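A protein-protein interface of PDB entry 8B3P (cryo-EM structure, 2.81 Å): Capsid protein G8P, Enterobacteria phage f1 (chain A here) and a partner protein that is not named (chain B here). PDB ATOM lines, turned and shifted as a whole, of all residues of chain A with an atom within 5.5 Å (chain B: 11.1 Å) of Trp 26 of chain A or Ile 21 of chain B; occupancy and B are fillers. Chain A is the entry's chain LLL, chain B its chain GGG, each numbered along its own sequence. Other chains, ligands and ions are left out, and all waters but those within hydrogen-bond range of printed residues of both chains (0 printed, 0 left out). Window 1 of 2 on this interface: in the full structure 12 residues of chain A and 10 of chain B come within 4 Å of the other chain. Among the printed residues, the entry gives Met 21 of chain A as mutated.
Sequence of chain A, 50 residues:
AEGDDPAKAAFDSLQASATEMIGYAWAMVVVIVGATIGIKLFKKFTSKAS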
ATOM      1  N   MET A  21       3.454 -23.354 -18.223  1.00  0.00           N
ATOM      2  CA  MET A  21       4.004 -22.518 -17.162  1.00  0.00           C
ATOM      3  C   MET A  21       3.160 -21.253 -17.001  1.00  0.00           C
ATOM      4  O   MET A  21       2.910 -20.820 -15.874  1.00  0.00           O
ATOM      5  CB  MET A  21       5.461 -22.126 -17.446  1.00  0.00           C
ATOM      6  CG  MET A  21       6.261 -21.674 -16.217  1.00  0.00           C
ATOM      7  SD  MET A  21       7.146 -20.100 -16.456  1.00  0.00           S
ATOM      8  CE  MET A  21       6.180 -18.995 -15.424  1.00  0.00           C
ATOM      9  N   ILE A  22       2.716 -20.678 -18.129  1.00  0.00           N
ATOM     10  CA  ILE A  22       1.898 -19.480 -18.107  1.00  0.00           C
ATOM     11  C   ILE A  22       0.576 -19.783 -17.410  1.00  0.00           C
ATOM     12  O   ILE A  22       0.035 -18.909 -16.747  1.00  0.00           O
ATOM     13  CB  ILE A  22       1.717 -18.883 -19.518  1.00  0.00           C
ATOM     14  CG1 ILE A  22       1.280 -17.418 -19.437  1.00  0.00           C
ATOM     15  CG2 ILE A  22       0.789 -19.713 -20.401  1.00  0.00           C
ATOM     16  CD1 ILE A  22       2.230 -16.546 -18.647  1.00  0.00           C
ATOM     17  N   GLY A  23       0.099 -21.029 -17.549  1.00  0.00           N
ATOM     18  CA  GLY A  23      -1.128 -21.499 -16.927  1.00  0.00           C
ATOM     19  C   GLY A  23      -1.034 -21.499 -15.403  1.00  0.00           C
ATOM     20  O   GLY A  23      -1.976 -21.082 -14.727  1.00  0.00           O
ATOM     21  N   TYR A  24       0.111 -21.961 -14.881  1.00  0.00           N
ATOM     22  CA  TYR A  24       0.332 -22.036 -13.446  1.00  0.00           C
ATOM     23  C   TYR A  24       0.449 -20.631 -12.858  1.00  0.00           C
ATOM     24  O   TYR A  24      -0.071 -20.371 -11.775  1.00  0.00           O
ATOM     25  CB  TYR A  24       1.590 -22.835 -13.095  1.00  0.00           C
ATOM     26  CG  TYR A  24       1.754 -24.212 -13.689  1.00  0.00           C
ATOM     27  CD1 TYR A  24       0.711 -25.131 -13.718  1.00  0.00           C
ATOM     28  CD2 TYR A  24       2.988 -24.611 -14.184  1.00  0.00           C
ATOM     29  CE1 TYR A  24       0.881 -26.396 -14.262  1.00  0.00           C
ATOM     30  CE2 TYR A  24       3.177 -25.875 -14.723  1.00  0.00           C
ATOM     31  CZ  TYR A  24       2.119 -26.769 -14.765  1.00  0.00           C
ATOM     32  OH  TYR A  24       2.304 -28.012 -15.301  1.00  0.00           O
ATOM     33  N   ALA A  25       1.143 -19.741 -13.581  1.00  0.00           N
ATOM     34  CA  ALA A  25       1.404 -18.380 -13.136  1.00  0.00           C
ATOM     35  C   ALA A  25       0.098 -17.600 -12.980  1.00  0.00           C
ATOM     36  O   ALA A  25      -0.050 -16.839 -12.031  1.00  0.00           O
ATOM     37  CB  ALA A  25       2.363 -17.697 -14.080  1.00  0.00           C
ATOM     38  N   TRP A  26      -0.855 -17.812 -13.899  1.00  0.00           N
ATOM     39  CA  TRP A  26      -2.133 -17.118 -13.853  1.00  0.00           C
ATOM     40  C   TRP A  26      -2.926 -17.524 -12.612  1.00  0.00           C
ATOM     41  O   TRP A  26      -3.638 -16.698 -12.053  1.00  0.00           O
ATOM     42  CB  TRP A  26      -2.938 -17.281 -15.152  1.00  0.00           C
ATOM     43  CG  TRP A  26      -2.725 -16.150 -16.114  1.00  0.00           C
ATOM     44  CD1 TRP A  26      -1.953 -16.153 -17.242  1.00  0.00           C
ATOM     45  CD2 TRP A  26      -3.272 -14.823 -16.014  1.00  0.00           C
ATOM     46  NE1 TRP A  26      -1.986 -14.929 -17.850  1.00  0.00           N
ATOM     47  CE2 TRP A  26      -2.786 -14.090 -17.121  1.00  0.00           C
ATOM     48  CE3 TRP A  26      -4.121 -14.181 -15.102  1.00  0.00           C
ATOM     49  CZ2 TRP A  26      -3.126 -12.754 -17.340  1.00  0.00           C
ATOM     50  CZ3 TRP A  26      -4.458 -12.860 -15.318  1.00  0.00           C
ATOM     51  CH2 TRP A  26      -3.964 -12.159 -16.422  1.00  0.00           C
ATOM     52  N   ALA A  27      -2.762 -18.780 -12.178  1.00  0.00           N
ATOM     53  CA  ALA A  27      -3.475 -19.317 -11.027  1.00  0.00           C
ATOM     54  C   ALA A  27      -2.995 -18.661  -9.731  1.00  0.00           C
ATOM     55  O   ALA A  27      -3.815 -18.266  -8.896  1.00  0.00           O
ATOM     56  CB  ALA A  27      -3.338 -20.821 -10.991  1.00  0.00           C
ATOM     57  N   MET A  28      -1.667 -18.533  -9.595  1.00  0.00           N
ATOM     58  CA  MET A  28      -1.030 -17.929  -8.431  1.00  0.00           C
ATOM     59  C   MET A  28      -1.461 -16.470  -8.300  1.00  0.00           C
ATOM     60  O   MET A  28      -1.889 -16.043  -7.224  1.00  0.00           O
ATOM     61  CB  MET A  28       0.503 -17.964  -8.523  1.00  0.00           C
ATOM     62  CG  MET A  28       1.166 -19.172  -7.883  1.00  0.00           C
ATOM     63  SD  MET A  28       0.441 -19.566  -6.284  1.00  0.00           S
ATOM     64  CE  MET A  28       1.102 -18.240  -5.283  1.00  0.00           C
ATOM     65  N   VAL A  29      -1.330 -15.724  -9.410  1.00  0.00           N
ATOM     66  CA  VAL A  29      -1.548 -14.284  -9.424  1.00  0.00           C
ATOM     67  C   VAL A  29      -2.952 -13.975  -8.916  1.00  0.00           C
ATOM     68  O   VAL A  29      -3.095 -13.070  -8.101  1.00  0.00           O
ATOM     69  CB  VAL A  29      -1.231 -13.633 -10.789  1.00  0.00           C
ATOM     70  CG1 VAL A  29      -1.818 -12.235 -10.959  1.00  0.00           C
ATOM     71  CG2 VAL A  29       0.269 -13.596 -11.037  1.00  0.00           C
ATOM     72  N   VAL A  30      -3.945 -14.772  -9.340  1.00  0.00           N
ATOM     73  CA  VAL A  30      -5.336 -14.506  -9.007  1.00  0.00           C
ATOM     74  C   VAL A  30      -5.514 -14.491  -7.488  1.00  0.00           C
ATOM     75  O   VAL A  30      -6.159 -13.579  -6.956  1.00  0.00           O
ATOM     76  CB  VAL A  30      -6.310 -15.462  -9.733  1.00  0.00           C
ATOM     77  CG1 VAL A  30      -7.694 -15.518  -9.095  1.00  0.00           C
ATOM     78  CG2 VAL A  30      -6.451 -15.089 -11.199  1.00  0.00           C
ATOM     79  N   LEU B  13       8.138 -14.088 -27.510  1.00  0.00           N
ATOM     80  CA  LEU B  13       7.103 -14.937 -26.937  1.00  0.00           C
ATOM     81  C   LEU B  13       7.048 -14.736 -25.422  1.00  0.00           C
ATOM     82  O   LEU B  13       5.960 -14.672 -24.849  1.00  0.00           O
ATOM     83  CB  LEU B  13       7.363 -16.402 -27.314  1.00  0.00           C
ATOM     84  CG  LEU B  13       6.316 -17.424 -26.864  1.00  0.00           C
ATOM     85  CD1 LEU B  13       5.130 -17.461 -27.817  1.00  0.00           C
ATOM     86  CD2 LEU B  13       6.936 -18.807 -26.735  1.00  0.00           C
ATOM     87  N   GLY B  14       8.229 -14.615 -24.801  1.00  0.00           N
ATOM     88  CA  GLY B  14       8.373 -14.442 -23.365  1.00  0.00           C
ATOM     89  C   GLY B  14       7.958 -13.047 -22.901  1.00  0.00           C
ATOM     90  O   GLY B  14       7.455 -12.904 -21.788  1.00  0.00           O
ATOM     91  N   TRP B  15       8.187 -12.038 -23.760  1.00  0.00           N
ATOM     92  CA  TRP B  15       7.808 -10.655 -23.493  1.00  0.00           C
ATOM     93  C   TRP B  15       6.284 -10.519 -23.449  1.00  0.00           C
ATOM     94  O   TRP B  15       5.754  -9.817 -22.590  1.00  0.00           O
ATOM     95  CB  TRP B  15       8.475  -9.671 -24.475  1.00  0.00           C
ATOM     96  CG  TRP B  15       8.098  -8.232 -24.265  1.00  0.00           C
ATOM     97  CD1 TRP B  15       8.654  -7.349 -23.383  1.00  0.00           C
ATOM     98  CD2 TRP B  15       7.060  -7.503 -24.951  1.00  0.00           C
ATOM     99  NE1 TRP B  15       8.035  -6.130 -23.466  1.00  0.00           N
ATOM    100  CE2 TRP B  15       7.049  -6.194 -24.415  1.00  0.00           C
ATOM    101  CE3 TRP B  15       6.138  -7.828 -25.958  1.00  0.00           C
ATOM    102  CZ2 TRP B  15       6.152  -5.221 -24.859  1.00  0.00           C
ATOM    103  CZ3 TRP B  15       5.246  -6.868 -26.388  1.00  0.00           C
ATOM    104  CH2 TRP B  15       5.259  -5.580 -25.848  1.00  0.00           C
ATOM    105  N   CYS B  16       5.590 -11.233 -24.343  1.00  0.00           N
ATOM    106  CA  CYS B  16       4.148 -11.116 -24.502  1.00  0.00           C
ATOM    107  C   CYS B  16       3.401 -11.792 -23.355  1.00  0.00           C
ATOM    108  O   CYS B  16       2.415 -11.247 -22.860  1.00  0.00           O
ATOM    109  CB  CYS B  16       3.701 -11.742 -25.815  1.00  0.00           C
ATOM    110  SG  CYS B  16       3.967 -10.643 -27.231  1.00  0.00           S
ATOM    111  N   LEU B  17       3.869 -12.989 -22.973  1.00  0.00           N
ATOM    112  CA  LEU B  17       3.189 -13.852 -22.018  1.00  0.00           C
ATOM    113  C   LEU B  17       3.192 -13.223 -20.625  1.00  0.00           C
ATOM    114  O   LEU B  17       2.187 -13.299 -19.917  1.00  0.00           O
ATOM    115  CB  LEU B  17       3.848 -15.238 -22.025  1.00  0.00           C
ATOM    116  CG  LEU B  17       3.607 -16.100 -23.268  1.00  0.00           C
ATOM    117  CD1 LEU B  17       4.349 -17.425 -23.168  1.00  0.00           C
ATOM    118  CD2 LEU B  17       2.124 -16.336 -23.520  1.00  0.00           C
ATOM    119  N   ARG B  18       4.317 -12.587 -20.265  1.00  0.00           N
ATOM    120  CA  ARG B  18       4.504 -11.988 -18.952  1.00  0.00           C
ATOM    121  C   ARG B  18       3.780 -10.646 -18.850  1.00  0.00           C
ATOM    122  O   ARG B  18       3.143 -10.385 -17.832  1.00  0.00           O
ATOM    123  CB  ARG B  18       5.989 -11.848 -18.596  1.00  0.00           C
ATOM    124  CG  ARG B  18       6.265 -11.194 -17.245  1.00  0.00           C
ATOM    125  CD  ARG B  18       5.813 -11.959 -16.010  1.00  0.00           C
ATOM    126  NE  ARG B  18       6.143 -11.283 -14.756  1.00  0.00           N
ATOM    127  CZ  ARG B  18       5.396 -10.363 -14.142  1.00  0.00           C
ATOM    128  NH1 ARG B  18       4.243  -9.967 -14.660  1.00  0.00           N
ATOM    129  NH2 ARG B  18       5.811  -9.828 -13.008  1.00  0.00           N
ATOM    130  N   SER B  19       3.894  -9.809 -19.893  1.00  0.00           N
ATOM    131  CA  SER B  19       3.353  -8.456 -19.873  1.00  0.00           C
ATOM    132  C   SER B  19       1.834  -8.472 -19.712  1.00  0.00           C
ATOM    133  O   SER B  19       1.280  -7.535 -19.139  1.00  0.00           O
ATOM    134  CB  SER B  19       3.783  -7.661 -21.074  1.00  0.00           C
ATOM    135  OG  SER B  19       3.472  -8.368 -22.261  1.00  0.00           O
ATOM    136  N   GLY B  20       1.196  -9.547 -20.209  1.00  0.00           N
ATOM    137  CA  GLY B  20      -0.198  -9.879 -19.948  1.00  0.00           C
ATOM    138  C   GLY B  20      -0.558  -9.731 -18.471  1.00  0.00           C
ATOM    139  O   GLY B  20      -1.536  -9.066 -18.141  1.00  0.00           O
ATOM    140  N   ILE B  21       0.290 -10.296 -17.602  1.00  0.00           N
ATOM    141  CA  ILE B  21       0.095 -10.274 -16.161  1.00  0.00           C
ATOM    142  C   ILE B  21       0.418  -8.888 -15.602  1.00  0.00           C
ATOM    143  O   ILE B  21      -0.243  -8.455 -14.660  1.00  0.00           O
ATOM    144  CB  ILE B  21       0.879 -11.412 -15.476  1.00  0.00           C
ATOM    145  CG1 ILE B  21       0.440 -12.770 -16.029  1.00  0.00           C
ATOM    146  CG2 ILE B  21       0.731 -11.363 -13.962  1.00  0.00           C
ATOM    147  CD1 ILE B  21       1.115 -13.960 -15.385  1.00  0.00           C
ATOM    148  N   THR B  22       1.402  -8.187 -16.188  1.00  0.00           N
ATOM    149  CA  THR B  22       1.764  -6.845 -15.742  1.00  0.00           C
ATOM    150  C   THR B  22       0.572  -5.898 -15.901  1.00  0.00           C
ATOM    151  O   THR B  22       0.387  -4.990 -15.089  1.00  0.00           O
ATOM    152  CB  THR B  22       3.049  -6.351 -16.425  1.00  0.00           C
ATOM    153  OG1 THR B  22       4.100  -7.261 -16.107  1.00  0.00           O
ATOM    154  CG2 THR B  22       3.483  -4.966 -15.999  1.00  0.00           C
ATOM    155  N   TYR B  23      -0.239  -6.132 -16.940  1.00  0.00           N
ATOM    156  CA  TYR B  23      -1.366  -5.265 -17.247  1.00  0.00           C
ATOM    157  C   TYR B  23      -2.537  -5.559 -16.310  1.00  0.00           C
ATOM    158  O   TYR B  23      -3.174  -4.623 -15.832  1.00  0.00           O
ATOM    159  CB  TYR B  23      -1.702  -5.295 -18.741  1.00  0.00           C
ATOM    160  CG  TYR B  23      -0.578  -4.863 -19.654  1.00  0.00           C
ATOM    161  CD1 TYR B  23       0.384  -3.947 -19.242  1.00  0.00           C
ATOM    162  CD2 TYR B  23      -0.483  -5.357 -20.948  1.00  0.00           C
ATOM    163  CE1 TYR B  23       1.419  -3.552 -20.078  1.00  0.00           C
ATOM    164  CE2 TYR B  23       0.546  -4.974 -21.797  1.00  0.00           C
ATOM    165  CZ  TYR B  23       1.499  -4.065 -21.364  1.00  0.00           C
ATOM    166  OH  TYR B  23       2.508  -3.680 -22.201  1.00  0.00           O
ATOM    167  N   PHE B  24      -2.790  -6.849 -16.036  1.00  0.00           N
ATOM    168  CA  PHE B  24      -3.810  -7.254 -15.078  1.00  0.00           C
ATOM    169  C   PHE B  24      -3.586  -6.533 -13.752  1.00  0.00           C
ATOM    170  O   PHE B  24      -4.427  -5.735 -13.350  1.00  0.00           O
ATOM    171  CB  PHE B  24      -3.863  -8.776 -14.918  1.00  0.00           C
ATOM    172  CG  PHE B  24      -4.879  -9.271 -13.917  1.00  0.00           C
ATOM    173  CD1 PHE B  24      -6.242  -9.194 -14.184  1.00  0.00           C
ATOM    174  CD2 PHE B  24      -4.477  -9.823 -12.705  1.00  0.00           C
ATOM    175  CE1 PHE B  24      -7.178  -9.647 -13.261  1.00  0.00           C
ATOM    176  CE2 PHE B  24      -5.414 -10.283 -11.786  1.00  0.00           C
ATOM    177  CZ  PHE B  24      -6.763 -10.197 -12.065  1.00  0.00           C
ATOM    178  N   THR B  25      -2.420  -6.766 -13.132  1.00  0.00           N
ATOM    179  CA  THR B  25      -2.074  -6.205 -11.831  1.00  0.00           C
ATOM    180  C   THR B  25      -2.273  -4.689 -11.815  1.00  0.00           C
ATOM    181  O   THR B  25      -2.890  -4.171 -10.888  1.00  0.00           O
ATOM    182  CB  THR B  25      -0.657  -6.593 -11.385  1.00  0.00           C
ATOM    183  OG1 THR B  25       0.253  -6.082 -12.358  1.00  0.00           O
ATOM    184  CG2 THR B  25      -0.454  -8.085 -11.225  1.00  0.00           C
ATOM    185  N   ARG B  26      -1.772  -3.997 -12.847  1.00  0.00           N
ATOM    186  CA  ARG B  26      -1.839  -2.544 -12.925  1.00  0.00           C
ATOM    187  C   ARG B  26      -3.287  -2.064 -12.962  1.00  0.00           C
ATOM    188  O   ARG B  26      -3.681  -1.242 -12.137  1.00  0.00           O
ATOM    189  CB  ARG B  26      -1.081  -2.018 -14.147  1.00  0.00           C
ATOM    190  CG  ARG B  26       0.406  -1.809 -13.912  1.00  0.00           C
ATOM    191  CD  ARG B  26       1.002  -0.948 -15.010  1.00  0.00           C
ATOM    192  NE  ARG B  26       1.937   0.036 -14.474  1.00  0.00           N
ATOM    193  CZ  ARG B  26       1.649   1.307 -14.191  1.00  0.00           C
ATOM    194  NH1 ARG B  26       0.434   1.787 -14.395  1.00  0.00           N
ATOM    195  NH2 ARG B  26       2.589   2.100 -13.704  1.00  0.00           N
ATOM    196  N   LEU B  27      -4.069  -2.582 -13.919  1.00  0.00           N
ATOM    197  CA  LEU B  27      -5.434  -2.127 -14.137  1.00  0.00           C
ATOM    198  C   LEU B  27      -6.260  -2.329 -12.870  1.00  0.00           C
ATOM    199  O   LEU B  27      -7.071  -1.474 -12.526  1.00  0.00           O
ATOM    200  CB  LEU B  27      -6.052  -2.840 -15.345  1.00  0.00           C
ATOM    201  CG  LEU B  27      -5.707  -2.249 -16.716  1.00  0.00           C
ATOM    202  CD1 LEU B  27      -6.004  -3.247 -17.826  1.00  0.00           C
ATOM    203  CD2 LEU B  27      -6.430  -0.931 -16.968  1.00  0.00           C
ATOM    204  N   MET B  28      -5.982  -3.427 -12.154  1.00  0.00           N
ATOM    205  CA  MET B  28      -6.665  -3.798 -10.927  1.00  0.00           C
ATOM    206  C   MET B  28      -6.370  -2.785  -9.820  1.00  0.00           C
ATOM    207  O   MET B  28      -7.300  -2.214  -9.259  1.00  0.00           O
ATOM    208  CB  MET B  28      -6.225  -5.189 -10.480  1.00  0.00           C
ATOM    209  CG  MET B  28      -7.091  -5.732  -9.385  1.00  0.00           C
ATOM    210  SD  MET B  28      -7.461  -7.471  -9.675  1.00  0.00           S
ATOM    211  CE  MET B  28      -8.713  -7.334 -10.943  1.00  0.00           C
ATOM    212  N   GLU B  29      -5.079  -2.572  -9.526  1.00  0.00           N
ATOM    213  CA  GLU B  29      -4.630  -1.650  -8.494  1.00  0.00           C
ATOM    214  C   GLU B  29      -5.292  -0.283  -8.655  1.00  0.00           C
ATOM    215  O   GLU B  29      -5.819   0.253  -7.684  1.00  0.00           O
ATOM    216  CB  GLU B  29      -3.109  -1.493  -8.508  1.00  0.00           C
ATOM    217  CG  GLU B  29      -2.370  -2.668  -7.890  1.00  0.00           C
ATOM    218  CD  GLU B  29      -0.887  -2.763  -8.218  1.00  0.00           C
ATOM    219  OE1 GLU B  29      -0.450  -3.849  -8.667  1.00  0.00           O
ATOM    220  OE2 GLU B  29      -0.164  -1.759  -8.013  1.00  0.00           O
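The side-chain hydroxyl of Thr 25 of chain B lies within hydrogen-bond range of the backbone carbonyl oxygen of Ile 21 of chain B, 3.3 Å away.
Among the printed residues, pairs that only touch across the chains: Ile 22 of chain A with Leu 17 of chain B, Trp 26 of chain A with Ile 21 of chain B, Trp 26 of chain A with Phe 24 of chain B, Val 29 of chain A with Ile 21 of chain B and Val 29 of chain A with Phe 24 of chain B.
Of chain B, only Ile 21 and Phe 24 come within 4 Å of Trp 26 of chain A.
Of chain A, only Trp 26 (3.7 Å) and Val 29 (3.7 Å) come within 4 Å of Ile 21 of chain B.
Of chain B, only Leu 17 (3.5 Å) comes within 4 Å of Ile 22 of chain A.
No residue of chain B comes within 4 Å of Gly 23 of chain A.
Of the printed residues of chain A, Phe 24 of chain B touches Trp 26 and Val 29.
Of the printed residues of chain B, Val 29 of chain A touches Ile 21 (3.7 Å) and Phe 24 (3.99 Å).
Leu 27 of chain B touches none of the printed residues of chain A.
The nearest residue of chain B that does not touch Trp 26 of chain A is Gly 20 of chain B (4.1 Å).
Of the 10 printed residues of chain A, 3 touch a printed residue of chain B.
Hydrophobic or aromatic side chains of chain A that line the printed part of chain B: Ile 22, Trp 26 and Val 29.
Of the 17 printed residues of chain B, 3 touch a printed residue of chain A.
Hydrophobic or aromatic side chains of chain B within 4 Å of the printed part of chain A: Leu 17, Ile 21 and Phe 24.
Among the printed residues, no Asp or Glu carboxylate lies within 4 Å of a Lys or Arg side-chain nitrogen of the other chain.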
